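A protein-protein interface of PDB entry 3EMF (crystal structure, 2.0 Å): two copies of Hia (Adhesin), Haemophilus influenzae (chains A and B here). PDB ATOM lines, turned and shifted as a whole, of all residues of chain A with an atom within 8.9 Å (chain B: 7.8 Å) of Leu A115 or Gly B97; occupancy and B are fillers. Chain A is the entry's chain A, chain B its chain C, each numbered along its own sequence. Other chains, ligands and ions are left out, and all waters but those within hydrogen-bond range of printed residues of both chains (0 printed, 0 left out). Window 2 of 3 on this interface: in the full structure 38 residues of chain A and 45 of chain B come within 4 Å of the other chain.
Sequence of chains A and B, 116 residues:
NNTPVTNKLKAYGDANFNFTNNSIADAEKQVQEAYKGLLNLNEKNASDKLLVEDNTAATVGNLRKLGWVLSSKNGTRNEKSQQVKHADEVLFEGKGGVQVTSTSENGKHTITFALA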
ATOM      1  N   LYS A  95      -1.605   0.712  13.061  1.00  0.00           N
ATOM      2  CA  LYS A  95      -1.983   1.982  13.669  1.00  0.00           C
ATOM      3  C   LYS A  95      -1.179   3.112  13.045  1.00  0.00           C
ATOM      4  O   LYS A  95      -0.458   2.903  12.074  1.00  0.00           O
ATOM      5  CB  LYS A  95      -1.790   1.946  15.184  1.00  0.00           C
ATOM      6  CG  LYS A  95      -0.404   1.524  15.623  1.00  0.00           C
ATOM      7  CD  LYS A  95      -0.333   1.462  17.138  1.00  0.00           C
ATOM      8  CE  LYS A  95       1.060   1.107  17.612  1.00  0.00           C
ATOM      9  NZ  LYS A  95       1.098   0.953  19.092  1.00  0.00           N
ATOM     10  N   GLY A  96      -1.319   4.313  13.589  1.00  0.00           N
ATOM     11  CA  GLY A  96      -0.534   5.439  13.124  1.00  0.00           C
ATOM     12  C   GLY A  96      -0.598   5.652  11.623  1.00  0.00           C
ATOM     13  O   GLY A  96       0.418   5.942  10.984  1.00  0.00           O
ATOM     14  N   GLY A  97      -1.791   5.509  11.053  1.00  0.00           N
ATOM     15  CA  GLY A  97      -1.989   5.827   9.652  1.00  0.00           C
ATOM     16  C   GLY A  97      -1.956   4.630   8.714  1.00  0.00           C
ATOM     17  O   GLY A  97      -2.062   4.787   7.500  1.00  0.00           O
ATOM     18  N   VAL A  98      -1.796   3.434   9.277  1.00  0.00           N
ATOM     19  CA  VAL A  98      -1.797   2.197   8.492  1.00  0.00           C
ATOM     20  C   VAL A  98      -2.973   1.322   8.914  1.00  0.00           C
ATOM     21  O   VAL A  98      -3.228   1.142  10.108  1.00  0.00           O
ATOM     22  CB  VAL A  98      -0.491   1.392   8.664  1.00  0.00           C
ATOM     23  CG1 VAL A  98      -0.540   0.115   7.843  1.00  0.00           C
ATOM     24  CG2 VAL A  98       0.713   2.219   8.269  1.00  0.00           C
ATOM     25  N   GLN A  99      -3.687   0.797   7.925  1.00  0.00           N
ATOM     26  CA  GLN A  99      -4.841  -0.066   8.152  1.00  0.00           C
ATOM     27  C   GLN A  99      -4.474  -1.521   7.825  1.00  0.00           C
ATOM     28  O   GLN A  99      -3.845  -1.801   6.807  1.00  0.00           O
ATOM     29  CB  GLN A  99      -6.011   0.395   7.274  1.00  0.00           C
ATOM     30  CG  GLN A  99      -7.387   0.077   7.845  1.00  0.00           C
ATOM     31  CD  GLN A  99      -8.524   0.618   6.991  1.00  0.00           C
ATOM     32  OE1 GLN A  99      -8.701   0.199   5.845  1.00  0.00           O
ATOM     33  NE2 GLN A  99      -9.312   1.542   7.555  1.00  0.00           N
ATOM     34  N   VAL A 100      -4.852  -2.439   8.703  1.00  0.00           N
ATOM     35  CA  VAL A 100      -4.586  -3.858   8.487  1.00  0.00           C
ATOM     36  C   VAL A 100      -5.871  -4.618   8.711  1.00  0.00           C
ATOM     37  O   VAL A 100      -6.490  -4.501   9.767  1.00  0.00           O
ATOM     38  CB  VAL A 100      -3.531  -4.423   9.476  1.00  0.00           C
ATOM     39  CG1 VAL A 100      -3.409  -5.930   9.303  1.00  0.00           C
ATOM     40  CG2 VAL A 100      -2.187  -3.742   9.284  1.00  0.00           C
ATOM     41  N   THR A 112      -4.342  -7.756   4.527  1.00  0.00           N
ATOM     42  CA  THR A 112      -4.340  -6.673   3.564  1.00  0.00           C
ATOM     43  C   THR A 112      -3.902  -5.382   4.221  1.00  0.00           C
ATOM     44  O   THR A 112      -4.365  -5.047   5.311  1.00  0.00           O
ATOM     45  CB  THR A 112      -5.749  -6.467   2.995  1.00  0.00           C
ATOM     46  OG1 THR A 112      -6.191  -7.680   2.381  1.00  0.00           O
ATOM     47  CG2 THR A 112      -5.759  -5.326   1.968  1.00  0.00           C
ATOM     48  N   PHE A 113      -3.022  -4.652   3.541  1.00  0.00           N
ATOM     49  CA  PHE A 113      -2.440  -3.439   4.096  1.00  0.00           C
ATOM     50  C   PHE A 113      -2.824  -2.237   3.261  1.00  0.00           C
ATOM     51  O   PHE A 113      -2.671  -2.253   2.047  1.00  0.00           O
ATOM     52  CB  PHE A 113      -0.919  -3.554   4.137  1.00  0.00           C
ATOM     53  CG  PHE A 113      -0.438  -4.700   4.947  1.00  0.00           C
ATOM     54  CD1 PHE A 113      -0.428  -5.981   4.415  1.00  0.00           C
ATOM     55  CD2 PHE A 113      -0.033  -4.513   6.255  1.00  0.00           C
ATOM     56  CE1 PHE A 113       0.000  -7.048   5.161  1.00  0.00           C
ATOM     57  CE2 PHE A 113       0.398  -5.576   7.003  1.00  0.00           C
ATOM     58  CZ  PHE A 113       0.416  -6.851   6.453  1.00  0.00           C
ATOM     59  N   ALA A 114      -3.311  -1.196   3.924  1.00  0.00           N
ATOM     60  CA  ALA A 114      -3.754   0.004   3.230  1.00  0.00           C
ATOM     61  C   ALA A 114      -3.499   1.228   4.103  1.00  0.00           C
ATOM     62  O   ALA A 114      -3.114   1.091   5.257  1.00  0.00           O
ATOM     63  CB  ALA A 114      -5.230  -0.114   2.877  1.00  0.00           C
ATOM     64  N   LEU A 115      -3.721   2.418   3.557  1.00  0.00           N
ATOM     65  CA  LEU A 115      -3.510   3.654   4.306  1.00  0.00           C
ATOM     66  C   LEU A 115      -4.699   3.996   5.197  1.00  0.00           C
ATOM     67  O   LEU A 115      -5.832   4.091   4.716  1.00  0.00           O
ATOM     68  CB  LEU A 115      -3.236   4.806   3.349  1.00  0.00           C
ATOM     69  CG  LEU A 115      -1.797   4.992   2.874  1.00  0.00           C
ATOM     70  CD1 LEU A 115      -1.110   3.662   2.666  1.00  0.00           C
ATOM     71  CD2 LEU A 115      -1.771   5.830   1.600  1.00  0.00           C
ATOM     72  N   ASN B  74      -7.242  -3.642  13.292  1.00  0.00           N
ATOM     73  CA  ASN B  74      -7.316  -2.350  12.648  1.00  0.00           C
ATOM     74  C   ASN B  74      -7.545  -1.262  13.693  1.00  0.00           C
ATOM     75  O   ASN B  74      -8.684  -0.968  14.048  1.00  0.00           O
ATOM     76  CB  ASN B  74      -8.451  -2.350  11.633  1.00  0.00           C
ATOM     77  CG  ASN B  74      -8.387  -1.170  10.705  1.00  0.00           C
ATOM     78  OD1 ASN B  74      -7.349  -0.518  10.596  1.00  0.00           O
ATOM     79  ND2 ASN B  74      -9.494  -0.882  10.029  1.00  0.00           N
ATOM     80  N   GLY B  94      -0.987  -5.871  -0.526  1.00  0.00           N
ATOM     81  CA  GLY B  94      -0.872  -4.433  -0.369  1.00  0.00           C
ATOM     82  C   GLY B  94      -1.833  -3.714  -1.295  1.00  0.00           C
ATOM     83  O   GLY B  94      -1.945  -4.072  -2.473  1.00  0.00           O
ATOM     84  N   LYS B  95      -2.537  -2.718  -0.764  1.00  0.00           N
ATOM     85  CA  LYS B  95      -3.363  -1.841  -1.595  1.00  0.00           C
ATOM     86  C   LYS B  95      -3.298  -0.379  -1.129  1.00  0.00           C
ATOM     87  O   LYS B  95      -2.748  -0.080  -0.070  1.00  0.00           O
ATOM     88  CB  LYS B  95      -4.813  -2.333  -1.629  1.00  0.00           C
ATOM     89  CG  LYS B  95      -5.431  -2.476  -0.253  1.00  0.00           C
ATOM     90  CD  LYS B  95      -6.852  -2.985  -0.325  1.00  0.00           C
ATOM     91  CE  LYS B  95      -6.932  -4.275  -1.129  1.00  0.00           C
ATOM     92  NZ  LYS B  95      -8.316  -4.834  -1.138  1.00  0.00           N
ATOM     93  N   GLY B  96      -3.870   0.512  -1.936  1.00  0.00           N
ATOM     94  CA  GLY B  96      -3.899   1.948  -1.690  1.00  0.00           C
ATOM     95  C   GLY B  96      -3.529   2.501  -0.321  1.00  0.00           C
ATOM     96  O   GLY B  96      -4.381   2.670   0.567  1.00  0.00           O
ATOM     97  N   GLY B  97      -2.251   2.825  -0.162  1.00  0.00           N
ATOM     98  CA  GLY B  97      -1.269   2.629  -1.209  1.00  0.00           C
ATOM     99  C   GLY B  97       0.015   2.088  -0.612  1.00  0.00           C
ATOM    100  O   GLY B  97       1.082   2.691  -0.724  1.00  0.00           O
ATOM    101  N   VAL B  98      -0.100   0.952   0.065  1.00  0.00           N
ATOM    102  CA  VAL B  98       1.066   0.253   0.573  1.00  0.00           C
ATOM    103  C   VAL B  98       1.540  -0.710  -0.498  1.00  0.00           C
ATOM    104  O   VAL B  98       0.734  -1.378  -1.145  1.00  0.00           O
ATOM    105  CB  VAL B  98       0.743  -0.537   1.850  1.00  0.00           C
ATOM    106  CG1 VAL B  98       1.965  -1.318   2.312  1.00  0.00           C
ATOM    107  CG2 VAL B  98       0.263   0.400   2.945  1.00  0.00           C
ATOM    108  N   GLN B  99       2.848  -0.773  -0.710  1.00  0.00           N
ATOM    109  CA  GLN B  99       3.373  -1.769  -1.629  1.00  0.00           C
ATOM    110  C   GLN B  99       3.920  -2.941  -0.824  1.00  0.00           C
ATOM    111  O   GLN B  99       4.727  -2.752   0.080  1.00  0.00           O
ATOM    112  CB  GLN B  99       4.448  -1.176  -2.537  1.00  0.00           C
ATOM    113  CG  GLN B  99       4.714  -2.000  -3.789  1.00  0.00           C
ATOM    114  CD  GLN B  99       5.698  -1.333  -4.736  1.00  0.00           C
ATOM    115  OE1 GLN B  99       6.759  -0.862  -4.316  1.00  0.00           O
ATOM    116  NE2 GLN B  99       5.353  -1.296  -6.022  1.00  0.00           N
ATOM    117  N   VAL B 100       3.447  -4.142  -1.141  1.00  0.00           N
ATOM    118  CA  VAL B 100       3.888  -5.358  -0.469  1.00  0.00           C
ATOM    119  C   VAL B 100       4.529  -6.293  -1.474  1.00  0.00           C
ATOM    120  O   VAL B 100       3.845  -6.911  -2.289  1.00  0.00           O
ATOM    121  CB  VAL B 100       2.719  -6.104   0.206  1.00  0.00           C
ATOM    122  CG1 VAL B 100       3.183  -7.463   0.700  1.00  0.00           C
ATOM    123  CG2 VAL B 100       2.158  -5.283   1.351  1.00  0.00           C
ATOM    124  N   ALA B 114       6.443  -0.854   1.608  1.00  0.00           N
ATOM    125  CA  ALA B 114       6.832   0.496   1.204  1.00  0.00           C
ATOM    126  C   ALA B 114       5.631   1.418   1.004  1.00  0.00           C
ATOM    127  O   ALA B 114       4.478   0.978   1.063  1.00  0.00           O
ATOM    128  CB  ALA B 114       7.670   0.447  -0.068  1.00  0.00           C
ATOM    129  N   LEU B 115       5.922   2.694   0.758  1.00  0.00           N
ATOM    130  CA  LEU B 115       4.906   3.713   0.498  1.00  0.00           C
ATOM    131  C   LEU B 115       4.047   3.971   1.731  1.00  0.00           C
ATOM    132  O   LEU B 115       4.404   4.781   2.588  1.00  0.00           O
ATOM    133  CB  LEU B 115       4.028   3.323  -0.696  1.00  0.00           C
ATOM    134  CG  LEU B 115       4.618   3.446  -2.100  1.00  0.00           C
ATOM    135  CD1 LEU B 115       6.112   3.175  -2.116  1.00  0.00           C
ATOM    136  CD2 LEU B 115       3.886   2.521  -3.069  1.00  0.00           C
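Of the 10 printed residues of chain B, 6 touch a printed residue of chain A. Hydrophobic or aromatic side chains of chain B within 4 Å of the printed part of chain A: Val B98. Hydrophobic or aromatic side chains of chain A within 4 Å of the printed part of chain B: Ala A114 and Leu A115. Among the printed residues, 11 pairs touch across the chains. Among the printed residues, no Asp or Glu carboxylate lies within 4 Å of a Lys or Arg side-chain nitrogen of the other chain.
Val A98 touches none of the printed residues of chain B. Of the printed residues of chain B, Gln A99 touches Asn B74. Of the printed residues of chain B, Val A100 touches Asn B74. Of chain B, only Lys B95 (3.5 Å) and Gly B96 (3.7 Å) come within 4 Å of Ala A114. Of chain B, only Gly B96 (3.1 Å), Gly B97 (3.2 Å) and Val B98 (3.6 Å) come within 4 Å of Leu A115. Of the printed residues of chain A, Gly B94 touches Phe A113. Gly B97 touches just one residue of chain A: Leu A115.
The backbone carbonyl oxygen of Phe A113 lies within hydrogen-bond range of the backbone NH of Lys B95. The backbone NH (N) of Leu A115 is in hydrogen-bond range of the backbone carbonyl oxygen (O) of Gly B96 (3.1 Å). The side-chain amide nitrogen (NE2) of Gln A99 lies close to the side-chain amide nitrogen (ND2) of Asn B74 (3.5 Å).
Among the printed residues, pairs that only touch across the chains: Leu A115 with Gly B97 (3.2 Å), Ala A114 with Lys B95 (3.5 Å), Thr A112 with Lys B95 (3.5 Å), Val A100 with Asn B74 (3.5 Å), Leu A115 with Val B98 (3.6 Å), Ala A114 with Gly B96 (3.7 Å), Phe A113 with Gly B94 (3.7 Å) and Phe A113 with Val B98 (3.8 Å).
Ala A114 touches Lys B95, but with the chains exchanged Lys A95 does not touch Ala B114 (12.2 Å). Ala A114 touches Gly B96, but with the chains exchanged Gly A96 does not touch Ala B114 (11.8 Å). Leu A115 touches Gly B97, but with the chains exchanged Gly A97 does not touch Leu B115 (8.1 Å). Leu A115 touches Val B98, but with the chains exchanged Val A98 does not touch Leu B115 (7.2 Å). Positions printed for both chains: 95, 96, 97, 98, 99, 100, 114 and 115.
N of Gln A99 lies within hydrogen-bond range of O of Ala A114, at 2.7 Å.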
